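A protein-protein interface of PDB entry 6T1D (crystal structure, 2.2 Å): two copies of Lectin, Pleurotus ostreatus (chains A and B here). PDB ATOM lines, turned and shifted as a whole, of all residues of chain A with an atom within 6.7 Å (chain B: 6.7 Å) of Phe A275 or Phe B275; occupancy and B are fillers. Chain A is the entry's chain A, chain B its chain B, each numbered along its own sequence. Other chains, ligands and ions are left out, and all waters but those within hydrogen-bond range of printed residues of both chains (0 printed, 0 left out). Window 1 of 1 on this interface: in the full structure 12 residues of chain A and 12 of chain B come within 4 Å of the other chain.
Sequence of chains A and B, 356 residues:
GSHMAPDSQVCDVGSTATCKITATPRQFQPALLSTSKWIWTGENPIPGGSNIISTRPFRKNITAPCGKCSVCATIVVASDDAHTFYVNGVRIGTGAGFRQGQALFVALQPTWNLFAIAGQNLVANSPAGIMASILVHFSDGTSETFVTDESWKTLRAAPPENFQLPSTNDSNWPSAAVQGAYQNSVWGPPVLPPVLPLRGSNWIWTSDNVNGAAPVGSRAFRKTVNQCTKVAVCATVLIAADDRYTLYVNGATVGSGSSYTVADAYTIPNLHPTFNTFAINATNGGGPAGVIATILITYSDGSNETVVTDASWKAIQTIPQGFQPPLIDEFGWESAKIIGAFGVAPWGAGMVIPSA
Among the printed residues, merely in contact across the chains: Asn A250 with Leu B327 (3.5 Å), His A272 with Leu B327 (3.5 Å), Thr A274 with Phe B275 (3.996 Å), Phe A275 with Thr B274 (3.9 Å), Phe A275 with Phe B275 (3.5 Å), Phe A275 with Leu B327 (3.4 Å), Pro A326 with Leu B327 (3.5 Å), Leu A327 with Asn B250 (3.3 Å), Leu A327 with His B272 (3.4 Å), Leu A327 with Phe B275 (3.3 Å) and Leu A327 with Pro B326 (3.6 Å).
Hydrophobic or aromatic side chains of chain A that line the printed part of chain B: His A272, Phe A275, Pro A326 and Leu A327.
Hydrophobic or aromatic side chains of chain B within 4 Å of the printed part of chain A: His B272, Phe B275, Pro B326 and Leu B327.
Among the printed residues, 12 pairs touch across the chains.
Among the printed residues, no Asp or Glu carboxylate lies within 4 Å of a Lys or Arg side-chain nitrogen of the other chain.
The side-chain amide oxygen of Asn B226 is in hydrogen-bond range of the side-chain amide nitrogen of Asn A226 (2.9 Å).
Of the printed residues of chain B, Asn A226 touches Asn B226 (2.9 Å).
Of the printed residues of chain B, Asn A250 touches Leu B327 (3.5 Å).
Phe A275 touches just these residues of chain B: Thr B274, Phe B275 and Leu B327.
Asn A276 touches none of the printed residues of chain B.
Printed residues of chain B within 4 Å of Leu A327: Asn B250, His B272, Phe B275 and Pro B326.
Of the printed residues of chain A, Asn B250 touches Leu A327.
Thr B277 touches none of the printed residues of chain A.
The nearest printed residue of chain A that does not touch Phe B275 is His A272 (4.4 Å).
ND2 of Asn B226 is in hydrogen-bond range of O of Thr B274, at 2.8 Å.
ND2 of Asn B250 is in hydrogen-bond range of OD1 of Asn B276.
The backbone NH of Phe A275 lies within hydrogen-bond range of a ring nitrogen (ND1) of His A272, at 3.3 Å.
The side-chain hydroxyl (OG1) of Thr A277 lies within hydrogen-bond range of the backbone carbonyl oxygen (O) of Pro A326 (3.4 Å).
A ring nitrogen (ND1) of His A272 sits close to the backbone NH (N) of Thr A274 (3.4 Å).
ND2 of Asn A250 is in hydrogen-bond range of OD1 of Asn A276 (3.0 Å).
Asn B226 touches its own counterpart, Asn A226.
Asn A250 touches Leu B327, and with the chains exchanged Leu A327 touches Asn B250.
Phe B275 touches its own counterpart, Phe A275.
Phe A275 touches Leu B327, and with the chains exchanged Leu A327 touches Phe B275.
Positions printed for both chains: 222, 224, 225, 226, 227, 232, 250, 271, 272, 273, 274, 275, 276, 277, 326 and 327.
Of the 12 pairs that touch across the chains among the printed residues, 12 have their exchanged pair printed and touching as well.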
ATOM      1  N   ARG A 222     -18.349  24.290 -28.610  1.00  0.00           N
ATOM      2  CA  ARG A 222     -18.240  23.564 -27.352  1.00  0.00           C
ATOM      3  C   ARG A 222     -19.423  23.909 -26.463  1.00  0.00           C
ATOM      4  O   ARG A 222     -19.960  25.021 -26.520  1.00  0.00           O
ATOM      5  CB  ARG A 222     -16.959  23.906 -26.587  1.00  0.00           C
ATOM      6  CG  ARG A 222     -15.688  23.683 -27.368  1.00  0.00           C
ATOM      7  CD  ARG A 222     -14.489  24.318 -26.684  1.00  0.00           C
ATOM      8  NE  ARG A 222     -14.392  23.918 -25.289  1.00  0.00           N
ATOM      9  CZ  ARG A 222     -13.820  22.786 -24.893  1.00  0.00           C
ATOM     10  NH1 ARG A 222     -13.319  21.948 -25.796  1.00  0.00           N
ATOM     11  NH2 ARG A 222     -13.761  22.483 -23.600  1.00  0.00           N
ATOM     12  N   THR A 224     -20.338  22.576 -22.286  1.00  0.00           N
ATOM     13  CA  THR A 224     -20.025  21.702 -21.167  1.00  0.00           C
ATOM     14  C   THR A 224     -21.204  21.601 -20.210  1.00  0.00           C
ATOM     15  O   THR A 224     -21.854  22.606 -19.901  1.00  0.00           O
ATOM     16  CB  THR A 224     -18.790  22.210 -20.429  1.00  0.00           C
ATOM     17  OG1 THR A 224     -17.669  22.187 -21.329  1.00  0.00           O
ATOM     18  CG2 THR A 224     -18.509  21.342 -19.213  1.00  0.00           C
ATOM     19  N   VAL A 225     -21.465  20.390 -19.724  1.00  0.00           N
ATOM     20  CA  VAL A 225     -22.496  20.139 -18.720  1.00  0.00           C
ATOM     21  C   VAL A 225     -21.811  19.598 -17.471  1.00  0.00           C
ATOM     22  O   VAL A 225     -21.122  18.569 -17.528  1.00  0.00           O
ATOM     23  CB  VAL A 225     -23.564  19.163 -19.234  1.00  0.00           C
ATOM     24  CG1 VAL A 225     -24.698  19.043 -18.229  1.00  0.00           C
ATOM     25  CG2 VAL A 225     -24.078  19.604 -20.627  1.00  0.00           C
ATOM     26  N   ASN A 226     -21.973  20.310 -16.348  1.00  0.00           N
ATOM     27  CA  ASN A 226     -21.253  20.000 -15.103  1.00  0.00           C
ATOM     28  C   ASN A 226     -22.175  20.232 -13.901  1.00  0.00           C
ATOM     29  O   ASN A 226     -22.149  21.273 -13.243  1.00  0.00           O
ATOM     30  CB  ASN A 226     -19.971  20.829 -15.024  1.00  0.00           C
ATOM     31  CG  ASN A 226     -19.284  20.733 -13.688  1.00  0.00           C
ATOM     32  OD1 ASN A 226     -18.964  21.754 -13.088  1.00  0.00           O
ATOM     33  ND2 ASN A 226     -19.038  19.515 -13.218  1.00  0.00           N
ATOM     34  N   GLN A 227     -22.996  19.236 -13.617  1.00  0.00           N
ATOM     35  CA  GLN A 227     -23.892  19.222 -12.465  1.00  0.00           C
ATOM     36  C   GLN A 227     -23.196  18.441 -11.350  1.00  0.00           C
ATOM     37  O   GLN A 227     -23.324  17.222 -11.248  1.00  0.00           O
ATOM     38  CB  GLN A 227     -25.226  18.603 -12.852  1.00  0.00           C
ATOM     39  CG  GLN A 227     -26.392  19.080 -12.017  1.00  0.00           C
ATOM     40  CD  GLN A 227     -26.821  20.477 -12.389  1.00  0.00           C
ATOM     41  OE1 GLN A 227     -26.867  20.824 -13.568  1.00  0.00           O
ATOM     42  NE2 GLN A 227     -27.137  21.290 -11.386  1.00  0.00           N
ATOM     43  N   ALA A 232     -24.116  11.773 -13.553  1.00  0.00           N
ATOM     44  CA  ALA A 232     -24.497  11.657 -14.952  1.00  0.00           C
ATOM     45  C   ALA A 232     -24.210  10.247 -15.460  1.00  0.00           C
ATOM     46  O   ALA A 232     -23.220   9.624 -15.069  1.00  0.00           O
ATOM     47  CB  ALA A 232     -23.751  12.700 -15.777  1.00  0.00           C
ATOM     48  N   ASN A 250     -16.176  14.443 -24.572  1.00  0.00           N
ATOM     49  CA  ASN A 250     -14.953  14.340 -23.767  1.00  0.00           C
ATOM     50  C   ASN A 250     -13.718  14.019 -24.611  1.00  0.00           C
ATOM     51  O   ASN A 250     -12.770  13.392 -24.136  1.00  0.00           O
ATOM     52  CB  ASN A 250     -15.130  13.328 -22.644  1.00  0.00           C
ATOM     53  CG  ASN A 250     -16.183  13.759 -21.664  1.00  0.00           C
ATOM     54  OD1 ASN A 250     -16.242  14.936 -21.296  1.00  0.00           O
ATOM     55  ND2 ASN A 250     -17.034  12.824 -21.244  1.00  0.00           N
ATOM     56  N   LEU A 271     -20.787   8.442 -20.194  1.00  0.00           N
ATOM     57  CA  LEU A 271     -20.538   9.787 -19.692  1.00  0.00           C
ATOM     58  C   LEU A 271     -19.656   9.746 -18.451  1.00  0.00           C
ATOM     59  O   LEU A 271     -19.768   8.851 -17.606  1.00  0.00           O
ATOM     60  CB  LEU A 271     -21.839  10.506 -19.343  1.00  0.00           C
ATOM     61  CG  LEU A 271     -22.735  10.982 -20.476  1.00  0.00           C
ATOM     62  CD1 LEU A 271     -23.852  11.801 -19.868  1.00  0.00           C
ATOM     63  CD2 LEU A 271     -21.971  11.765 -21.523  1.00  0.00           C
ATOM     64  N   HIS A 272     -18.776  10.723 -18.340  1.00  0.00           N
ATOM     65  CA  HIS A 272     -18.140  10.960 -17.060  1.00  0.00           C
ATOM     66  C   HIS A 272     -19.211  11.384 -16.054  1.00  0.00           C
ATOM     67  O   HIS A 272     -20.166  12.082 -16.422  1.00  0.00           O
ATOM     68  CB  HIS A 272     -17.049  12.016 -17.222  1.00  0.00           C
ATOM     69  CG  HIS A 272     -16.240  12.247 -15.990  1.00  0.00           C
ATOM     70  ND1 HIS A 272     -16.537  13.245 -15.086  1.00  0.00           N
ATOM     71  CD2 HIS A 272     -15.155  11.602 -15.502  1.00  0.00           C
ATOM     72  CE1 HIS A 272     -15.655  13.218 -14.103  1.00  0.00           C
ATOM     73  NE2 HIS A 272     -14.804  12.232 -14.332  1.00  0.00           N
ATOM     74  N   PRO A 273     -19.132  10.934 -14.801  1.00  0.00           N
ATOM     75  CA  PRO A 273     -20.273  11.137 -13.890  1.00  0.00           C
ATOM     76  C   PRO A 273     -20.545  12.583 -13.469  1.00  0.00           C
ATOM     77  O   PRO A 273     -21.683  12.863 -13.073  1.00  0.00           O
ATOM     78  CB  PRO A 273     -19.929  10.247 -12.687  1.00  0.00           C
ATOM     79  CG  PRO A 273     -18.456   9.995 -12.788  1.00  0.00           C
ATOM     80  CD  PRO A 273     -18.148   9.984 -14.258  1.00  0.00           C
ATOM     81  N   THR A 274     -19.596  13.522 -13.572  1.00  0.00           N
ATOM     82  CA  THR A 274     -19.913  14.884 -13.126  1.00  0.00           C
ATOM     83  C   THR A 274     -19.638  15.952 -14.189  1.00  0.00           C
ATOM     84  O   THR A 274     -20.277  17.012 -14.163  1.00  0.00           O
ATOM     85  CB  THR A 274     -19.153  15.275 -11.843  1.00  0.00           C
ATOM     86  OG1 THR A 274     -17.785  15.567 -12.141  1.00  0.00           O
ATOM     87  CG2 THR A 274     -19.186  14.180 -10.836  1.00  0.00           C
ATOM     88  N   PHE A 275     -18.692  15.713 -15.107  1.00  0.00           N
ATOM     89  CA  PHE A 275     -18.214  16.748 -16.024  1.00  0.00           C
ATOM     90  C   PHE A 275     -18.091  16.167 -17.421  1.00  0.00           C
ATOM     91  O   PHE A 275     -17.327  15.222 -17.621  1.00  0.00           O
ATOM     92  CB  PHE A 275     -16.861  17.287 -15.544  1.00  0.00           C
ATOM     93  CG  PHE A 275     -16.342  18.474 -16.319  1.00  0.00           C
ATOM     94  CD1 PHE A 275     -15.664  18.298 -17.522  1.00  0.00           C
ATOM     95  CD2 PHE A 275     -16.479  19.764 -15.819  1.00  0.00           C
ATOM     96  CE1 PHE A 275     -15.165  19.386 -18.233  1.00  0.00           C
ATOM     97  CE2 PHE A 275     -15.968  20.856 -16.528  1.00  0.00           C
ATOM     98  CZ  PHE A 275     -15.310  20.656 -17.732  1.00  0.00           C
ATOM     99  N   ASN A 276     -18.840  16.717 -18.384  1.00  0.00           N
ATOM    100  CA  ASN A 276     -18.823  16.232 -19.762  1.00  0.00           C
ATOM    101  C   ASN A 276     -18.872  17.400 -20.728  1.00  0.00           C
ATOM    102  O   ASN A 276     -19.687  18.311 -20.550  1.00  0.00           O
ATOM    103  CB  ASN A 276     -20.014  15.335 -20.069  1.00  0.00           C
ATOM    104  CG  ASN A 276     -20.073  14.125 -19.182  1.00  0.00           C
ATOM    105  OD1 ASN A 276     -19.391  13.118 -19.423  1.00  0.00           O
ATOM    106  ND2 ASN A 276     -20.922  14.198 -18.151  1.00  0.00           N
ATOM    107  N   THR A 277     -18.033  17.345 -21.771  1.00  0.00           N
ATOM    108  CA  THR A 277     -17.910  18.396 -22.783  1.00  0.00           C
ATOM    109  C   THR A 277     -18.230  17.825 -24.156  1.00  0.00           C
ATOM    110  O   THR A 277     -17.606  16.848 -24.583  1.00  0.00           O
ATOM    111  CB  THR A 277     -16.504  18.995 -22.787  1.00  0.00           C
ATOM    112  OG1 THR A 277     -16.355  19.914 -21.701  1.00  0.00           O
ATOM    113  CG2 THR A 277     -16.222  19.698 -24.105  1.00  0.00           C
ATOM    114  N   PRO A 326     -11.846  17.957 -22.978  1.00  0.00           N
ATOM    115  CA  PRO A 326     -12.810  18.523 -22.022  1.00  0.00           C
ATOM    116  C   PRO A 326     -12.365  19.836 -21.408  1.00  0.00           C
ATOM    117  O   PRO A 326     -13.081  20.841 -21.473  1.00  0.00           O
ATOM    118  CB  PRO A 326     -12.921  17.434 -20.950  1.00  0.00           C
ATOM    119  CG  PRO A 326     -12.406  16.169 -21.611  1.00  0.00           C
ATOM    120  CD  PRO A 326     -11.356  16.632 -22.558  1.00  0.00           C
ATOM    121  N   LEU A 327     -11.192  19.843 -20.793  1.00  0.00           N
ATOM    122  CA  LEU A 327     -10.647  21.053 -20.198  1.00  0.00           C
ATOM    123  C   LEU A 327      -9.696  21.698 -21.188  1.00  0.00           C
ATOM    124  O   LEU A 327      -8.654  21.126 -21.525  1.00  0.00           O
ATOM    125  CB  LEU A 327      -9.928  20.774 -18.884  1.00  0.00           C
ATOM    126  CG  LEU A 327     -10.768  20.404 -17.687  1.00  0.00           C
ATOM    127  CD1 LEU A 327      -9.896  20.509 -16.458  1.00  0.00           C
ATOM    128  CD2 LEU A 327     -11.855  21.441 -17.638  1.00  0.00           C
ATOM    129  N   ARG B 222      -4.886  10.924  -7.238  1.00  0.00           N
ATOM    130  CA  ARG B 222      -5.676  11.981  -7.852  1.00  0.00           C
ATOM    131  C   ARG B 222      -6.662  12.548  -6.841  1.00  0.00           C
ATOM    132  O   ARG B 222      -7.178  11.832  -5.973  1.00  0.00           O
ATOM    133  CB  ARG B 222      -6.442  11.457  -9.058  1.00  0.00           C
ATOM    134  CG  ARG B 222      -5.564  10.825 -10.108  1.00  0.00           C
ATOM    135  CD  ARG B 222      -6.398  10.032 -11.099  1.00  0.00           C
ATOM    136  NE  ARG B 222      -7.507  10.812 -11.638  1.00  0.00           N
ATOM    137  CZ  ARG B 222      -7.363  11.634 -12.664  1.00  0.00           C
ATOM    138  NH1 ARG B 222      -6.166  11.761 -13.218  1.00  0.00           N
ATOM    139  NH2 ARG B 222      -8.391  12.333 -13.126  1.00  0.00           N
ATOM    140  N   THR B 224      -9.796  15.656  -7.315  1.00  0.00           N
ATOM    141  CA  THR B 224     -10.457  16.665  -8.127  1.00  0.00           C
ATOM    142  C   THR B 224     -11.251  17.624  -7.248  1.00  0.00           C
ATOM    143  O   THR B 224     -11.861  17.213  -6.254  1.00  0.00           O
ATOM    144  CB  THR B 224     -11.364  16.013  -9.157  1.00  0.00           C
ATOM    145  OG1 THR B 224     -10.556  15.243 -10.045  1.00  0.00           O
ATOM    146  CG2 THR B 224     -12.125  17.057  -9.937  1.00  0.00           C
ATOM    147  N   VAL B 225     -11.191  18.907  -7.598  1.00  0.00           N
ATOM    148  CA  VAL B 225     -11.970  19.963  -6.964  1.00  0.00           C
ATOM    149  C   VAL B 225     -12.865  20.562  -8.036  1.00  0.00           C
ATOM    150  O   VAL B 225     -12.371  21.098  -9.038  1.00  0.00           O
ATOM    151  CB  VAL B 225     -11.061  21.033  -6.341  1.00  0.00           C
ATOM    152  CG1 VAL B 225     -11.871  22.036  -5.555  1.00  0.00           C
ATOM    153  CG2 VAL B 225     -10.000  20.380  -5.455  1.00  0.00           C
ATOM    154  N   ASN B 226     -14.179  20.465  -7.834  1.00  0.00           N
ATOM    155  CA  ASN B 226     -15.153  20.871  -8.845  1.00  0.00           C
ATOM    156  C   ASN B 226     -16.321  21.541  -8.127  1.00  0.00           C
ATOM    157  O   ASN B 226     -17.354  20.921  -7.872  1.00  0.00           O
ATOM    158  CB  ASN B 226     -15.614  19.673  -9.673  1.00  0.00           C
ATOM    159  CG  ASN B 226     -16.748  20.016 -10.605  1.00  0.00           C
ATOM    160  OD1 ASN B 226     -17.779  19.342 -10.629  1.00  0.00           O
ATOM    161  ND2 ASN B 226     -16.570  21.075 -11.380  1.00  0.00           N
ATOM    162  N   GLN B 227     -16.149  22.819  -7.795  1.00  0.00           N
ATOM    163  CA  GLN B 227     -17.184  23.605  -7.120  1.00  0.00           C
ATOM    164  C   GLN B 227     -17.915  24.403  -8.198  1.00  0.00           C
ATOM    165  O   GLN B 227     -17.567  25.544  -8.504  1.00  0.00           O
ATOM    166  CB  GLN B 227     -16.555  24.494  -6.058  1.00  0.00           C
ATOM    167  CG  GLN B 227     -17.458  24.741  -4.887  1.00  0.00           C
ATOM    168  CD  GLN B 227     -17.516  23.523  -3.995  1.00  0.00           C
ATOM    169  OE1 GLN B 227     -16.488  22.882  -3.741  1.00  0.00           O
ATOM    170  NE2 GLN B 227     -18.716  23.177  -3.533  1.00  0.00           N
ATOM    171  N   ALA B 232     -13.170  29.439  -9.639  1.00  0.00           N
ATOM    172  CA  ALA B 232     -11.862  29.204  -9.056  1.00  0.00           C
ATOM    173  C   ALA B 232     -10.818  30.032  -9.794  1.00  0.00           C
ATOM    174  O   ALA B 232     -10.913  30.221 -11.009  1.00  0.00           O
ATOM    175  CB  ALA B 232     -11.532  27.712  -9.114  1.00  0.00           C
ATOM    176  N   ASN B 250      -4.415  19.599 -13.871  1.00  0.00           N
ATOM    177  CA  ASN B 250      -5.132  19.451 -15.140  1.00  0.00           C
ATOM    178  C   ASN B 250      -4.266  18.823 -16.229  1.00  0.00           C
ATOM    179  O   ASN B 250      -4.434  19.124 -17.411  1.00  0.00           O
ATOM    180  CB  ASN B 250      -5.698  20.780 -15.628  1.00  0.00           C
ATOM    181  CG  ASN B 250      -6.723  21.326 -14.696  1.00  0.00           C
ATOM    182  OD1 ASN B 250      -7.547  20.569 -14.180  1.00  0.00           O
ATOM    183  ND2 ASN B 250      -6.696  22.644 -14.469  1.00  0.00           N
ATOM    184  N   LEU B 271      -5.714  28.218 -13.053  1.00  0.00           N
ATOM    185  CA  LEU B 271      -6.716  27.194 -12.796  1.00  0.00           C
ATOM    186  C   LEU B 271      -7.883  27.332 -13.753  1.00  0.00           C
ATOM    187  O   LEU B 271      -8.348  28.436 -14.051  1.00  0.00           O
ATOM    188  CB  LEU B 271      -7.253  27.269 -11.372  1.00  0.00           C
ATOM    189  CG  LEU B 271      -6.494  26.793 -10.148  1.00  0.00           C
ATOM    190  CD1 LEU B 271      -7.402  26.928  -8.961  1.00  0.00           C
ATOM    191  CD2 LEU B 271      -6.090  25.350 -10.321  1.00  0.00           C
ATOM    192  N   HIS B 272      -8.397  26.198 -14.183  1.00  0.00           N
ATOM    193  CA  HIS B 272      -9.688  26.197 -14.833  1.00  0.00           C
ATOM    194  C   HIS B 272     -10.743  26.706 -13.856  1.00  0.00           C
ATOM    195  O   HIS B 272     -10.700  26.372 -12.664  1.00  0.00           O
ATOM    196  CB  HIS B 272     -10.027  24.787 -15.293  1.00  0.00           C
ATOM    197  CG  HIS B 272     -11.285  24.704 -16.085  1.00  0.00           C
ATOM    198  ND1 HIS B 272     -12.509  24.455 -15.505  1.00  0.00           N
ATOM    199  CD2 HIS B 272     -11.514  24.839 -17.410  1.00  0.00           C
ATOM    200  CE1 HIS B 272     -13.440  24.438 -16.441  1.00  0.00           C
ATOM    201  NE2 HIS B 272     -12.861  24.665 -17.606  1.00  0.00           N
ATOM    202  N   PRO B 273     -11.697  27.513 -14.321  1.00  0.00           N
ATOM    203  CA  PRO B 273     -12.617  28.188 -13.390  1.00  0.00           C
ATOM    204  C   PRO B 273     -13.591  27.273 -12.652  1.00  0.00           C
ATOM    205  O   PRO B 273     -14.152  27.705 -11.637  1.00  0.00           O
ATOM    206  CB  PRO B 273     -13.374  29.167 -14.296  1.00  0.00           C
ATOM    207  CG  PRO B 273     -13.193  28.640 -15.679  1.00  0.00           C
ATOM    208  CD  PRO B 273     -11.842  28.012 -15.696  1.00  0.00           C
ATOM    209  N   THR B 274     -13.820  26.040 -13.103  1.00  0.00           N
ATOM    210  CA  THR B 274     -14.826  25.211 -12.450  1.00  0.00           C
ATOM    211  C   THR B 274     -14.317  23.830 -12.058  1.00  0.00           C
ATOM    212  O   THR B 274     -14.832  23.234 -11.101  1.00  0.00           O
ATOM    213  CB  THR B 274     -16.027  24.991 -13.367  1.00  0.00           C
ATOM    214  OG1 THR B 274     -15.662  24.024 -14.354  1.00  0.00           O
ATOM    215  CG2 THR B 274     -16.444  26.268 -14.083  1.00  0.00           C
ATOM    216  N   PHE B 275     -13.355  23.286 -12.811  1.00  0.00           N
ATOM    217  CA  PHE B 275     -12.962  21.882 -12.673  1.00  0.00           C
ATOM    218  C   PHE B 275     -11.447  21.778 -12.733  1.00  0.00           C
ATOM    219  O   PHE B 275     -10.843  22.169 -13.735  1.00  0.00           O
ATOM    220  CB  PHE B 275     -13.619  21.044 -13.779  1.00  0.00           C
ATOM    221  CG  PHE B 275     -13.450  19.556 -13.618  1.00  0.00           C
ATOM    222  CD1 PHE B 275     -12.291  18.925 -14.040  1.00  0.00           C
ATOM    223  CD2 PHE B 275     -14.473  18.784 -13.084  1.00  0.00           C
ATOM    224  CE1 PHE B 275     -12.143  17.555 -13.901  1.00  0.00           C
ATOM    225  CE2 PHE B 275     -14.333  17.411 -12.948  1.00  0.00           C
ATOM    226  CZ  PHE B 275     -13.166  16.798 -13.352  1.00  0.00           C
ATOM    227  N   ASN B 276     -10.824  21.279 -11.667  1.00  0.00           N
ATOM    228  CA  ASN B 276      -9.371  21.150 -11.624  1.00  0.00           C
ATOM    229  C   ASN B 276      -9.004  19.848 -10.938  1.00  0.00           C
ATOM    230  O   ASN B 276      -9.523  19.557  -9.858  1.00  0.00           O
ATOM    231  CB  ASN B 276      -8.734  22.311 -10.870  1.00  0.00           C
ATOM    232  CG  ASN B 276      -9.005  23.629 -11.528  1.00  0.00           C
ATOM    233  OD1 ASN B 276      -8.309  24.021 -12.461  1.00  0.00           O
ATOM    234  ND2 ASN B 276     -10.044  24.319 -11.068  1.00  0.00           N
ATOM    235  N   THR B 277      -8.051  19.115 -11.522  1.00  0.00           N
ATOM    236  CA  THR B 277      -7.634  17.796 -11.041  1.00  0.00           C
ATOM    237  C   THR B 277      -6.162  17.819 -10.661  1.00  0.00           C
ATOM    238  O   THR B 277      -5.314  18.161 -11.496  1.00  0.00           O
ATOM    239  CB  THR B 277      -7.851  16.735 -12.119  1.00  0.00           C
ATOM    240  OG1 THR B 277      -9.242  16.388 -12.193  1.00  0.00           O
ATOM    241  CG2 THR B 277      -6.987  15.493 -11.829  1.00  0.00           C
ATOM    242  N   PRO B 326      -7.316  15.324 -16.703  1.00  0.00           N
ATOM    243  CA  PRO B 326      -8.360  15.683 -15.718  1.00  0.00           C
ATOM    244  C   PRO B 326      -9.489  14.671 -15.659  1.00  0.00           C
ATOM    245  O   PRO B 326      -9.869  14.220 -14.571  1.00  0.00           O
ATOM    246  CB  PRO B 326      -8.844  17.054 -16.210  1.00  0.00           C
ATOM    247  CG  PRO B 326      -7.741  17.560 -17.101  1.00  0.00           C
ATOM    248  CD  PRO B 326      -7.138  16.357 -17.737  1.00  0.00           C
ATOM    249  N   LEU B 327     -10.066  14.344 -16.810  1.00  0.00           N
ATOM    250  CA  LEU B 327     -11.146  13.379 -16.924  1.00  0.00           C
ATOM    251  C   LEU B 327     -10.564  12.040 -17.335  1.00  0.00           C
ATOM    252  O   LEU B 327      -9.973  11.929 -18.414  1.00  0.00           O
ATOM    253  CB  LEU B 327     -12.168  13.835 -17.959  1.00  0.00           C
ATOM    254  CG  LEU B 327     -12.932  15.095 -17.613  1.00  0.00           C
ATOM    255  CD1 LEU B 327     -14.093  15.211 -18.558  1.00  0.00           C
ATOM    256  CD2 LEU B 327     -13.417  14.951 -16.202  1.00  0.00           C
